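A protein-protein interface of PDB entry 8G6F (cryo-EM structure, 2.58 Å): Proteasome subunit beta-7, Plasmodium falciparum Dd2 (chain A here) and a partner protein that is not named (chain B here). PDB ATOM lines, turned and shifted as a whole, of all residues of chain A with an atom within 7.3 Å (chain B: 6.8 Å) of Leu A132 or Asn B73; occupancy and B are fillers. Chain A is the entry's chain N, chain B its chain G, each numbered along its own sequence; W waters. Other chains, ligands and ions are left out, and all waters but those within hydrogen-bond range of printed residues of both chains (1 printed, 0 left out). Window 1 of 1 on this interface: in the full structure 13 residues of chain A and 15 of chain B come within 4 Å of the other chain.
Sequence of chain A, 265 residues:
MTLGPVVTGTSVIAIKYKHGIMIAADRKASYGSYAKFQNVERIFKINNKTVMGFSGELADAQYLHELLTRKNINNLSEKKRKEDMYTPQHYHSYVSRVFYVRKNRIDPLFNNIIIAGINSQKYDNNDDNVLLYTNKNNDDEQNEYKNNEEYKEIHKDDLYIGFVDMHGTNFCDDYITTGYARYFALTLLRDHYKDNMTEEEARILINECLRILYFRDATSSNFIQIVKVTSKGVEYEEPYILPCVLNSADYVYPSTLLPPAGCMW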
ATOM      1  N   LYS A  45     -14.661  32.498   1.315  1.00  0.00           N
ATOM      2  CA  LYS A  45     -13.693  31.508   1.760  1.00  0.00           C
ATOM      3  C   LYS A  45     -12.398  31.690   0.981  1.00  0.00           C
ATOM      4  O   LYS A  45     -12.404  31.640  -0.252  1.00  0.00           O
ATOM      5  CB  LYS A  45     -14.242  30.098   1.561  1.00  0.00           C
ATOM      6  CG  LYS A  45     -13.311  29.013   2.036  1.00  0.00           C
ATOM      7  CD  LYS A  45     -13.924  27.645   1.872  1.00  0.00           C
ATOM      8  CE  LYS A  45     -13.194  26.810   0.855  1.00  0.00           C
ATOM      9  NZ  LYS A  45     -13.534  25.375   1.020  1.00  0.00           N
ATOM     10  N   ILE A  46     -11.294  31.909   1.691  1.00  0.00           N
ATOM     11  CA  ILE A  46      -9.989  31.995   1.049  1.00  0.00           C
ATOM     12  C   ILE A  46      -9.380  30.614   0.872  1.00  0.00           C
ATOM     13  O   ILE A  46      -8.947  30.248  -0.222  1.00  0.00           O
ATOM     14  CB  ILE A  46      -9.056  32.920   1.855  1.00  0.00           C
ATOM     15  CG1 ILE A  46      -9.726  34.270   2.110  1.00  0.00           C
ATOM     16  CG2 ILE A  46      -7.748  33.122   1.115  1.00  0.00           C
ATOM     17  CD1 ILE A  46      -8.950  35.149   3.049  1.00  0.00           C
ATOM     18  N   ASN A  47      -9.340  29.833   1.944  1.00  0.00           N
ATOM     19  CA  ASN A  47      -8.974  28.426   1.870  1.00  0.00           C
ATOM     20  C   ASN A  47      -9.749  27.695   2.961  1.00  0.00           C
ATOM     21  O   ASN A  47     -10.717  28.227   3.510  1.00  0.00           O
ATOM     22  CB  ASN A  47      -7.449  28.246   1.970  1.00  0.00           C
ATOM     23  CG  ASN A  47      -6.865  28.827   3.232  1.00  0.00           C
ATOM     24  OD1 ASN A  47      -7.571  29.083   4.199  1.00  0.00           O
ATOM     25  ND2 ASN A  47      -5.557  29.024   3.234  1.00  0.00           N
ATOM     26  N   ASN A  48      -9.332  26.470   3.272  1.00  0.00           N
ATOM     27  CA  ASN A  48     -10.069  25.626   4.201  1.00  0.00           C
ATOM     28  C   ASN A  48     -10.037  26.137   5.634  1.00  0.00           C
ATOM     29  O   ASN A  48     -10.781  25.616   6.469  1.00  0.00           O
ATOM     30  CB  ASN A  48      -9.509  24.207   4.168  1.00  0.00           C
ATOM     31  CG  ASN A  48     -10.066  23.391   3.032  1.00  0.00           C
ATOM     32  OD1 ASN A  48     -11.162  23.651   2.548  1.00  0.00           O
ATOM     33  ND2 ASN A  48      -9.309  22.397   2.593  1.00  0.00           N
ATOM     34  N   THR A  69      -8.199  34.923  -3.888  1.00  0.00           N
ATOM     35  CA  THR A  69      -8.441  33.647  -4.548  1.00  0.00           C
ATOM     36  C   THR A  69      -7.226  33.211  -5.347  1.00  0.00           C
ATOM     37  O   THR A  69      -6.814  32.045  -5.294  1.00  0.00           O
ATOM     38  CB  THR A  69      -9.667  33.757  -5.453  1.00  0.00           C
ATOM     39  OG1 THR A  69     -10.852  33.791  -4.653  1.00  0.00           O
ATOM     40  CG2 THR A  69      -9.742  32.582  -6.409  1.00  0.00           C
ATOM     41  N   ARG A  70      -6.624  34.136  -6.089  1.00  0.00           N
ATOM     42  CA  ARG A  70      -5.461  33.750  -6.875  1.00  0.00           C
ATOM     43  C   ARG A  70      -4.247  33.491  -5.992  1.00  0.00           C
ATOM     44  O   ARG A  70      -3.441  32.601  -6.293  1.00  0.00           O
ATOM     45  CB  ARG A  70      -5.160  34.816  -7.921  1.00  0.00           C
ATOM     46  CG  ARG A  70      -5.937  34.605  -9.206  1.00  0.00           C
ATOM     47  CD  ARG A  70      -5.606  33.271  -9.845  1.00  0.00           C
ATOM     48  NE  ARG A  70      -6.713  32.325  -9.793  1.00  0.00           N
ATOM     49  CZ  ARG A  70      -6.715  31.139 -10.387  1.00  0.00           C
ATOM     50  NH1 ARG A  70      -5.677  30.712 -11.085  1.00  0.00           N
ATOM     51  NH2 ARG A  70      -7.787  30.361 -10.277  1.00  0.00           N
ATOM     52  N   ASN A  72      -4.401  32.131  -3.055  1.00  0.00           N
ATOM     53  CA  ASN A  72      -4.625  30.779  -2.559  1.00  0.00           C
ATOM     54  C   ASN A  72      -4.324  29.738  -3.627  1.00  0.00           C
ATOM     55  O   ASN A  72      -3.779  28.673  -3.326  1.00  0.00           O
ATOM     56  CB  ASN A  72      -6.059  30.624  -2.070  1.00  0.00           C
ATOM     57  CG  ASN A  72      -6.382  29.200  -1.685  1.00  0.00           C
ATOM     58  OD1 ASN A  72      -5.794  28.655  -0.759  1.00  0.00           O
ATOM     59  ND2 ASN A  72      -7.307  28.586  -2.405  1.00  0.00           N
ATOM     60  N   ILE A  73      -4.695  30.012  -4.877  1.00  0.00           N
ATOM     61  CA  ILE A  73      -4.428  29.045  -5.938  1.00  0.00           C
ATOM     62  C   ILE A  73      -2.929  28.847  -6.115  1.00  0.00           C
ATOM     63  O   ILE A  73      -2.455  27.723  -6.299  1.00  0.00           O
ATOM     64  CB  ILE A  73      -5.101  29.486  -7.250  1.00  0.00           C
ATOM     65  CG1 ILE A  73      -6.607  29.234  -7.173  1.00  0.00           C
ATOM     66  CG2 ILE A  73      -4.495  28.752  -8.430  1.00  0.00           C
ATOM     67  CD1 ILE A  73      -7.003  27.820  -7.493  1.00  0.00           C
ATOM     68  N   LEU A  76      -1.634  26.742  -3.295  1.00  0.00           N
ATOM     69  CA  LEU A  76      -1.985  25.342  -3.489  1.00  0.00           C
ATOM     70  C   LEU A  76      -1.125  24.700  -4.567  1.00  0.00           C
ATOM     71  O   LEU A  76      -0.759  23.526  -4.461  1.00  0.00           O
ATOM     72  CB  LEU A  76      -3.466  25.236  -3.846  1.00  0.00           C
ATOM     73  CG  LEU A  76      -4.159  23.901  -3.598  1.00  0.00           C
ATOM     74  CD1 LEU A  76      -3.917  23.409  -2.184  1.00  0.00           C
ATOM     75  CD2 LEU A  76      -5.642  24.049  -3.871  1.00  0.00           C
ATOM     76  N   SER A  77      -0.806  25.451  -5.621  1.00  0.00           N
ATOM     77  CA  SER A  77       0.067  24.933  -6.665  1.00  0.00           C
ATOM     78  C   SER A  77       1.436  24.582  -6.104  1.00  0.00           C
ATOM     79  O   SER A  77       2.002  23.535  -6.435  1.00  0.00           O
ATOM     80  CB  SER A  77       0.200  25.954  -7.790  1.00  0.00           C
ATOM     81  OG  SER A  77      -0.971  25.996  -8.581  1.00  0.00           O
ATOM     82  N   MET A  85       0.397  25.483   3.560  1.00  0.00           N
ATOM     83  CA  MET A  85      -0.739  26.355   3.305  1.00  0.00           C
ATOM     84  C   MET A  85      -0.633  27.630   4.129  1.00  0.00           C
ATOM     85  O   MET A  85      -0.231  27.605   5.293  1.00  0.00           O
ATOM     86  CB  MET A  85      -2.045  25.630   3.622  1.00  0.00           C
ATOM     87  CG  MET A  85      -2.462  24.603   2.577  1.00  0.00           C
ATOM     88  SD  MET A  85      -2.550  25.263   0.903  1.00  0.00           S
ATOM     89  CE  MET A  85      -4.258  25.778   0.827  1.00  0.00           C
ATOM     90  N   ASN A 129      -5.504  16.889   1.288  1.00  0.00           N
ATOM     91  CA  ASN A 129      -6.064  16.830  -0.059  1.00  0.00           C
ATOM     92  C   ASN A 129      -7.099  17.935  -0.176  1.00  0.00           C
ATOM     93  O   ASN A 129      -8.200  17.818   0.369  1.00  0.00           O
ATOM     94  CB  ASN A 129      -6.687  15.466  -0.348  1.00  0.00           C
ATOM     95  CG  ASN A 129      -5.671  14.349  -0.324  1.00  0.00           C
ATOM     96  OD1 ASN A 129      -5.017  14.070  -1.326  1.00  0.00           O
ATOM     97  ND2 ASN A 129      -5.533  13.702   0.823  1.00  0.00           N
ATOM     98  N   VAL A 130      -6.749  18.999  -0.884  1.00  0.00           N
ATOM     99  CA  VAL A 130      -7.601  20.175  -0.992  1.00  0.00           C
ATOM    100  C   VAL A 130      -8.513  20.013  -2.197  1.00  0.00           C
ATOM    101  O   VAL A 130      -8.053  19.699  -3.301  1.00  0.00           O
ATOM    102  CB  VAL A 130      -6.757  21.452  -1.107  1.00  0.00           C
ATOM    103  CG1 VAL A 130      -7.650  22.675  -1.235  1.00  0.00           C
ATOM    104  CG2 VAL A 130      -5.834  21.581   0.090  1.00  0.00           C
ATOM    105  N   LEU A 131      -9.807  20.216  -1.984  1.00  0.00           N
ATOM    106  CA  LEU A 131     -10.795  20.226  -3.051  1.00  0.00           C
ATOM    107  C   LEU A 131     -11.346  21.639  -3.171  1.00  0.00           C
ATOM    108  O   LEU A 131     -11.840  22.200  -2.188  1.00  0.00           O
ATOM    109  CB  LEU A 131     -11.915  19.225  -2.772  1.00  0.00           C
ATOM    110  CG  LEU A 131     -11.482  17.765  -2.610  1.00  0.00           C
ATOM    111  CD1 LEU A 131     -12.648  16.921  -2.152  1.00  0.00           C
ATOM    112  CD2 LEU A 131     -10.907  17.212  -3.899  1.00  0.00           C
ATOM    113  N   LEU A 132     -11.256  22.211  -4.368  1.00  0.00           N
ATOM    114  CA  LEU A 132     -11.697  23.577  -4.602  1.00  0.00           C
ATOM    115  C   LEU A 132     -13.097  23.670  -5.181  1.00  0.00           C
ATOM    116  O   LEU A 132     -13.787  24.663  -4.941  1.00  0.00           O
ATOM    117  CB  LEU A 132     -10.737  24.290  -5.558  1.00  0.00           C
ATOM    118  CG  LEU A 132      -9.300  24.474  -5.094  1.00  0.00           C
ATOM    119  CD1 LEU A 132      -8.469  25.005  -6.237  1.00  0.00           C
ATOM    120  CD2 LEU A 132      -9.244  25.407  -3.904  1.00  0.00           C
ATOM    121  N   TYR A 133     -13.526  22.671  -5.945  1.00  0.00           N
ATOM    122  CA  TYR A 133     -14.766  22.744  -6.700  1.00  0.00           C
ATOM    123  C   TYR A 133     -15.820  21.767  -6.207  1.00  0.00           C
ATOM    124  O   TYR A 133     -16.936  21.761  -6.736  1.00  0.00           O
ATOM    125  CB  TYR A 133     -14.472  22.506  -8.182  1.00  0.00           C
ATOM    126  CG  TYR A 133     -13.152  23.099  -8.615  1.00  0.00           C
ATOM    127  CD1 TYR A 133     -13.024  24.459  -8.843  1.00  0.00           C
ATOM    128  CD2 TYR A 133     -12.029  22.304  -8.775  1.00  0.00           C
ATOM    129  CE1 TYR A 133     -11.827  25.007  -9.226  1.00  0.00           C
ATOM    130  CE2 TYR A 133     -10.826  22.844  -9.160  1.00  0.00           C
ATOM    131  CZ  TYR A 133     -10.730  24.195  -9.384  1.00  0.00           C
ATOM    132  OH  TYR A 133      -9.530  24.741  -9.771  1.00  0.00           O
ATOM    133  N   THR A 134     -15.502  20.947  -5.212  1.00  0.00           N
ATOM    134  CA  THR A 134     -16.461  20.046  -4.592  1.00  0.00           C
ATOM    135  C   THR A 134     -16.287  20.131  -3.086  1.00  0.00           C
ATOM    136  O   THR A 134     -15.171  19.972  -2.579  1.00  0.00           O
ATOM    137  CB  THR A 134     -16.262  18.603  -5.073  1.00  0.00           C
ATOM    138  OG1 THR A 134     -16.702  18.488  -6.432  1.00  0.00           O
ATOM    139  CG2 THR A 134     -17.039  17.626  -4.205  1.00  0.00           C
ATOM    140  N   ASN A 135     -17.380  20.388  -2.376  1.00  0.00           N
ATOM    141  CA  ASN A 135     -17.368  20.493  -0.920  1.00  0.00           C
ATOM    142  C   ASN A 135     -17.957  19.207  -0.351  1.00  0.00           C
ATOM    143  O   ASN A 135     -19.173  19.011  -0.360  1.00  0.00           O
ATOM    144  CB  ASN A 135     -18.150  21.718  -0.457  1.00  0.00           C
ATOM    145  CG  ASN A 135     -17.797  22.133   0.957  1.00  0.00           C
ATOM    146  OD1 ASN A 135     -18.664  22.214   1.826  1.00  0.00           O
ATOM    147  ND2 ASN A 135     -16.519  22.405   1.195  1.00  0.00           N
ATOM    148  N   HIS B  71       0.484  20.531 -10.869  1.00  0.00           N
ATOM    149  CA  HIS B  71      -0.872  20.832 -11.290  1.00  0.00           C
ATOM    150  C   HIS B  71      -0.999  22.326 -11.524  1.00  0.00           C
ATOM    151  O   HIS B  71      -0.204  23.123 -11.021  1.00  0.00           O
ATOM    152  CB  HIS B  71      -1.910  20.353 -10.267  1.00  0.00           C
ATOM    153  CG  HIS B  71      -1.920  21.134  -8.992  1.00  0.00           C
ATOM    154  ND1 HIS B  71      -1.304  20.688  -7.844  1.00  0.00           N
ATOM    155  CD2 HIS B  71      -2.482  22.324  -8.678  1.00  0.00           C
ATOM    156  CE1 HIS B  71      -1.482  21.572  -6.881  1.00  0.00           C
ATOM    157  NE2 HIS B  71      -2.192  22.575  -7.362  1.00  0.00           N
ATOM    158  N   VAL B  72      -2.001  22.697 -12.315  1.00  0.00           N
ATOM    159  CA  VAL B  72      -2.209  24.104 -12.636  1.00  0.00           C
ATOM    160  C   VAL B  72      -3.312  24.684 -11.759  1.00  0.00           C
ATOM    161  O   VAL B  72      -3.064  25.595 -10.960  1.00  0.00           O
ATOM    162  CB  VAL B  72      -2.527  24.300 -14.128  1.00  0.00           C
ATOM    163  CG1 VAL B  72      -3.154  25.659 -14.366  1.00  0.00           C
ATOM    164  CG2 VAL B  72      -1.265  24.151 -14.949  1.00  0.00           C
ATOM    165  N   ASN B  73      -4.531  24.166 -11.891  1.00  0.00           N
ATOM    166  CA  ASN B  73      -5.674  24.680 -11.147  1.00  0.00           C
ATOM    167  C   ASN B  73      -6.205  23.668 -10.141  1.00  0.00           C
ATOM    168  O   ASN B  73      -7.331  23.811  -9.661  1.00  0.00           O
ATOM    169  CB  ASN B  73      -6.787  25.097 -12.108  1.00  0.00           C
ATOM    170  CG  ASN B  73      -6.629  26.512 -12.605  1.00  0.00           C
ATOM    171  OD1 ASN B  73      -6.234  27.401 -11.859  1.00  0.00           O
ATOM    172  ND2 ASN B  73      -6.941  26.730 -13.871  1.00  0.00           N
ATOM    173  N   ASN B  74      -5.415  22.653  -9.813  1.00  0.00           N
ATOM    174  CA  ASN B  74      -5.776  21.511  -8.989  1.00  0.00           C
ATOM    175  C   ASN B  74      -6.565  20.489  -9.794  1.00  0.00           C
ATOM    176  O   ASN B  74      -6.919  19.446  -9.248  1.00  0.00           O
ATOM    177  CB  ASN B  74      -6.589  21.903  -7.745  1.00  0.00           C
ATOM    178  CG  ASN B  74      -6.285  21.027  -6.547  1.00  0.00           C
ATOM    179  OD1 ASN B  74      -5.170  20.541  -6.384  1.00  0.00           O
ATOM    180  ND2 ASN B  74      -7.282  20.823  -5.701  1.00  0.00           N
ATOM    181  N   ASN B  75      -6.851  20.747 -11.070  1.00  0.00           N
ATOM    182  CA  ASN B  75      -7.541  19.782 -11.915  1.00  0.00           C
ATOM    183  C   ASN B  75      -6.870  19.619 -13.272  1.00  0.00           C
ATOM    184  O   ASN B  75      -7.466  19.020 -14.172  1.00  0.00           O
ATOM    185  CB  ASN B  75      -9.009  20.181 -12.103  1.00  0.00           C
ATOM    186  CG  ASN B  75      -9.171  21.585 -12.635  1.00  0.00           C
ATOM    187  OD1 ASN B  75      -8.207  22.227 -13.035  1.00  0.00           O
ATOM    188  ND2 ASN B  75     -10.402  22.072 -12.638  1.00  0.00           N
ATOM    189  N   ILE B  76      -5.656  20.134 -13.446  1.00  0.00           N
ATOM    190  CA  ILE B  76      -4.883  19.950 -14.667  1.00  0.00           C
ATOM    191  C   ILE B  76      -3.504  19.449 -14.269  1.00  0.00           C
ATOM    192  O   ILE B  76      -2.747  20.176 -13.617  1.00  0.00           O
ATOM    193  CB  ILE B  76      -4.763  21.249 -15.481  1.00  0.00           C
ATOM    194  CG1 ILE B  76      -6.129  21.689 -16.000  1.00  0.00           C
ATOM    195  CG2 ILE B  76      -3.794  21.068 -16.636  1.00  0.00           C
ATOM    196  CD1 ILE B  76      -6.155  23.117 -16.479  1.00  0.00           C
ATOM    197  N   ILE B  77      -3.179  18.225 -14.671  1.00  0.00           N
ATOM    198  CA  ILE B  77      -1.847  17.667 -14.471  1.00  0.00           C
ATOM    199  C   ILE B  77      -0.916  18.217 -15.537  1.00  0.00           C
ATOM    200  O   ILE B  77      -1.299  18.359 -16.701  1.00  0.00           O
ATOM    201  CB  ILE B  77      -1.887  16.130 -14.526  1.00  0.00           C
ATOM    202  CG1 ILE B  77      -2.385  15.551 -13.205  1.00  0.00           C
ATOM    203  CG2 ILE B  77      -0.508  15.574 -14.852  1.00  0.00           C
ATOM    204  CD1 ILE B  77      -2.649  14.066 -13.251  1.00  0.00           C
ATOM    205  N   ARG B  95       0.909  28.518 -15.103  1.00  0.00           N
ATOM    206  CA  ARG B  95       0.183  29.026 -13.946  1.00  0.00           C
ATOM    207  C   ARG B  95      -0.155  30.501 -14.113  1.00  0.00           C
ATOM    208  O   ARG B  95      -1.243  30.944 -13.732  1.00  0.00           O
ATOM    209  CB  ARG B  95       1.003  28.798 -12.681  1.00  0.00           C
ATOM    210  CG  ARG B  95       0.855  27.408 -12.129  1.00  0.00           C
ATOM    211  CD  ARG B  95       2.091  26.962 -11.399  1.00  0.00           C
ATOM    212  NE  ARG B  95       1.958  25.594 -10.916  1.00  0.00           N
ATOM    213  CZ  ARG B  95       2.873  24.964 -10.197  1.00  0.00           C
ATOM    214  NH1 ARG B  95       4.011  25.546  -9.864  1.00  0.00           N
ATOM    215  NH2 ARG B  95       2.638  23.720  -9.796  1.00  0.00           N
ATOM    216  N   ALA B  98      -3.109  30.744 -16.456  1.00  0.00           N
ATOM    217  CA  ALA B  98      -4.333  30.371 -15.754  1.00  0.00           C
ATOM    218  C   ALA B  98      -4.805  31.497 -14.843  1.00  0.00           C
ATOM    219  O   ALA B  98      -6.004  31.806 -14.788  1.00  0.00           O
ATOM    220  CB  ALA B  98      -4.107  29.091 -14.954  1.00  0.00           C
ATOM    221  N   ASN B  99      -3.876  32.129 -14.125  1.00  0.00           N
ATOM    222  CA  ASN B  99      -4.255  33.225 -13.241  1.00  0.00           C
ATOM    223  C   ASN B  99      -4.835  34.389 -14.025  1.00  0.00           C
ATOM    224  O   ASN B  99      -5.841  34.979 -13.620  1.00  0.00           O
ATOM    225  CB  ASN B  99      -3.051  33.693 -12.428  1.00  0.00           C
ATOM    226  CG  ASN B  99      -2.606  32.678 -11.411  1.00  0.00           C
ATOM    227  OD1 ASN B  99      -3.328  31.736 -11.098  1.00  0.00           O
ATOM    228  ND2 ASN B  99      -1.409  32.866 -10.881  1.00  0.00           N
ATOM    229  N   TYR B 102      -8.381  33.550 -15.207  1.00  0.00           N
ATOM    230  CA  TYR B 102      -9.365  33.668 -14.139  1.00  0.00           C
ATOM    231  C   TYR B 102      -9.624  35.129 -13.782  1.00  0.00           C
ATOM    232  O   TYR B 102     -10.771  35.516 -13.539  1.00  0.00           O
ATOM    233  CB  TYR B 102      -8.920  32.891 -12.906  1.00  0.00           C
ATOM    234  CG  TYR B 102      -9.978  32.874 -11.833  1.00  0.00           C
ATOM    235  CD1 TYR B 102     -10.033  33.869 -10.869  1.00  0.00           C
ATOM    236  CD2 TYR B 102     -10.940  31.878 -11.799  1.00  0.00           C
ATOM    237  CE1 TYR B 102     -11.004  33.864  -9.899  1.00  0.00           C
ATOM    238  CE2 TYR B 102     -11.914  31.866 -10.835  1.00  0.00           C
ATOM    239  CZ  TYR B 102     -11.942  32.861  -9.886  1.00  0.00           C
ATOM    240  OH  TYR B 102     -12.914  32.850  -8.916  1.00  0.00           O
ATOM    241  N   THR B 107     -13.508  32.335 -14.676  1.00  0.00           N
ATOM    242  CA  THR B 107     -13.626  30.894 -14.825  1.00  0.00           C
ATOM    243  C   THR B 107     -12.237  30.331 -15.061  1.00  0.00           C
ATOM    244  O   THR B 107     -11.291  31.063 -15.355  1.00  0.00           O
ATOM    245  CB  THR B 107     -14.566  30.503 -15.974  1.00  0.00           C
ATOM    246  OG1 THR B 107     -14.336  31.353 -17.101  1.00  0.00           O
ATOM    247  CG2 THR B 107     -16.015  30.622 -15.546  1.00  0.00           C
ATOM    248  N   ASN B 108     -12.114  29.017 -14.912  1.00  0.00           N
ATOM    249  CA  ASN B 108     -10.840  28.356 -15.152  1.00  0.00           C
ATOM    250  C   ASN B 108     -10.543  28.292 -16.643  1.00  0.00           C
ATOM    251  O   ASN B 108     -11.444  28.116 -17.465  1.00  0.00           O
ATOM    252  CB  ASN B 108     -10.859  26.950 -14.565  1.00  0.00           C
ATOM    253  CG  ASN B 108     -10.684  26.945 -13.070  1.00  0.00           C
ATOM    254  OD1 ASN B 108     -10.264  27.936 -12.478  1.00  0.00           O
ATOM    255  ND2 ASN B 108     -11.002  25.821 -12.448  1.00  0.00           N
ATOM    256  N   ILE B 109      -9.268  28.424 -16.988  1.00  0.00           N
ATOM    257  CA  ILE B 109      -8.867  28.423 -18.400  1.00  0.00           C
ATOM    258  C   ILE B 109      -9.149  27.051 -19.003  1.00  0.00           C
ATOM    259  O   ILE B 109      -8.816  26.027 -18.382  1.00  0.00           O
ATOM    260  CB  ILE B 109      -7.386  28.792 -18.534  1.00  0.00           C
ATOM    261  CG1 ILE B 109      -7.025  29.016 -20.004  1.00  0.00           C
ATOM    262  CG2 ILE B 109      -6.500  27.710 -17.941  1.00  0.00           C
ATOM    263  CD1 ILE B 109      -5.737  29.759 -20.205  1.00  0.00           C
ATOM    264  N   LEU B 114      -5.164  26.751 -22.840  1.00  0.00           N
ATOM    265  CA  LEU B 114      -3.892  26.761 -22.131  1.00  0.00           C
ATOM    266  C   LEU B 114      -2.806  26.078 -22.950  1.00  0.00           C
ATOM    267  O   LEU B 114      -1.662  26.544 -22.995  1.00  0.00           O
ATOM    268  CB  LEU B 114      -4.042  26.086 -20.770  1.00  0.00           C
ATOM    269  CG  LEU B 114      -2.795  26.096 -19.882  1.00  0.00           C
ATOM    270  CD1 LEU B 114      -2.462  27.500 -19.428  1.00  0.00           C
ATOM    271  CD2 LEU B 114      -2.985  25.183 -18.693  1.00  0.00           C
ATOM    272  N   GLU B 228      -9.923  15.922  -9.076  1.00  0.00           N
ATOM    273  CA  GLU B 228      -8.932  16.925  -8.735  1.00  0.00           C
ATOM    274  C   GLU B 228      -7.579  16.247  -8.613  1.00  0.00           C
ATOM    275  O   GLU B 228      -7.486  15.050  -8.338  1.00  0.00           O
ATOM    276  CB  GLU B 228      -9.288  17.646  -7.435  1.00  0.00           C
ATOM    277  CG  GLU B 228     -10.654  18.296  -7.459  1.00  0.00           C
ATOM    278  CD  GLU B 228     -10.678  19.666  -6.820  1.00  0.00           C
ATOM    279  OE1 GLU B 228      -9.609  20.289  -6.679  1.00  0.00           O
ATOM    280  OE2 GLU B 228     -11.776  20.118  -6.444  1.00  0.00           O
ATOM    281  N   PHE B 229      -6.527  17.025  -8.834  1.00  0.00           N
ATOM    282  CA  PHE B 229      -5.178  16.479  -8.824  1.00  0.00           C
ATOM    283  C   PHE B 229      -4.887  15.810  -7.491  1.00  0.00           C
ATOM    284  O   PHE B 229      -5.155  16.375  -6.429  1.00  0.00           O
ATOM    285  CB  PHE B 229      -4.167  17.590  -9.083  1.00  0.00           C
ATOM    286  CG  PHE B 229      -2.746  17.158  -8.924  1.00  0.00           C
ATOM    287  CD1 PHE B 229      -2.115  16.440  -9.917  1.00  0.00           C
ATOM    288  CD2 PHE B 229      -2.040  17.467  -7.778  1.00  0.00           C
ATOM    289  CE1 PHE B 229      -0.815  16.043  -9.772  1.00  0.00           C
ATOM    290  CE2 PHE B 229      -0.740  17.069  -7.630  1.00  0.00           C
ATOM    291  CZ  PHE B 229      -0.125  16.357  -8.629  1.00  0.00           C
HETATM  292  O   HOH W   1     -13.886  18.291  -7.512  1.00  0.00           O
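The guanidinium group of Arg A70 lies within hydrogen-bond range of the side-chain amide oxygen of Asn B73 (3.4 Å). The guanidinium group (NH1) of Arg A70 lies within hydrogen-bond range of the side-chain amide oxygen (OD1) of Asn B99, at 2.6 Å. The backbone carbonyl oxygen (O) of Leu A76 lies close to a ring nitrogen (NE2) of His B71. O of Val B72 is in hydrogen-bond range of OG of Ser A77 (3.2 Å). NH2 of Arg B95 lies within hydrogen-bond range of O of Ser A77, 3.4 Å away. ND2 of Asn B74 lies within hydrogen-bond range of O of Val A130, at 2.8 Å. N of Leu A132 is in hydrogen-bond range of OE2 of Glu B228, at 3.0 Å. The side-chain hydroxyl of Tyr A133 lies within hydrogen-bond range of the side-chain amide nitrogen of Asn B108. The side-chain carboxylate (OE2) of Glu B228 lies within hydrogen-bond range of the backbone NH (N) of Tyr A133, at 3.1 Å. The backbone carbonyl oxygen (O) of Asn B73 sits close to the side-chain hydroxyl (OH) of Tyr A133.
The backbone carbonyl oxygen (O) of Ile A73 lies within hydrogen-bond range of the side-chain hydroxyl (OG) of Ser A77, at 3.2 Å. The backbone carbonyl oxygen (O) of His B71 sits at hydrogen-bond distance from the guanidinium group (NH2) of Arg B95, 3.2 Å away. The side-chain amide nitrogen (ND2) of Asn B74 is in hydrogen-bond range of the side-chain carboxylate (OE1) of Glu B228, 2.6 Å away. The backbone carbonyl oxygen (O) of Asn B74 is in hydrogen-bond range of the backbone NH (N) of Phe B229 (2.5 Å). The backbone carbonyl oxygen of Arg B95 sits close to the side-chain amide nitrogen of Asn B99, 3.4 Å away.
Tyr B102 touches Thr A69. Arg A70 touches Ala B98. NH2 of Arg A70 touches CG of Tyr B102, 3.7 Å away. CA of Ser A77 touches NE2 of His B71 (3.3 Å). Val A130 touches Glu B228. OE2 of Glu B228 touches CA of Leu A131, at 3.5 Å. Leu A132 touches Asn B73. Leu A132 touches Asn B74. ND2 of Asn B75 touches CE2 of Tyr A133, at 3.6 Å.
Of chain B, only Asn B73, Asn B74 and Glu B228 come within 4 Å of Leu A132. Asn B73 touches three residues of chain A. Printed residues of chain B within 4 Å of Tyr A133: Asn B73, Asn B75, Asn B108 and Glu B228. Printed residues of chain A within 4 Å of Asn B75: Tyr A133. Printed residues of chain A within 4 Å of Ala B98: Arg A70 (3.9 Å). Of the printed residues of chain B, Ser A77 touches His B71 (3.3 Å), Val B72 (3.2 Å) and Arg B95 (3.4 Å). The nearest residue of chain B that does not touch Leu A132 is Asn B75 (6.6 Å).
Of the 18 printed residues of chain A, 8 touch a printed residue of chain B. Along chain A the printed residues that touch a printed residue of chain B span positions 69 to 133.
Water W1 bridges the side-chain carboxylate (OE2) of Glu B228 (3.0 Å) and the side-chain hydroxyl (OG1) of Thr A134 (3.0 Å).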
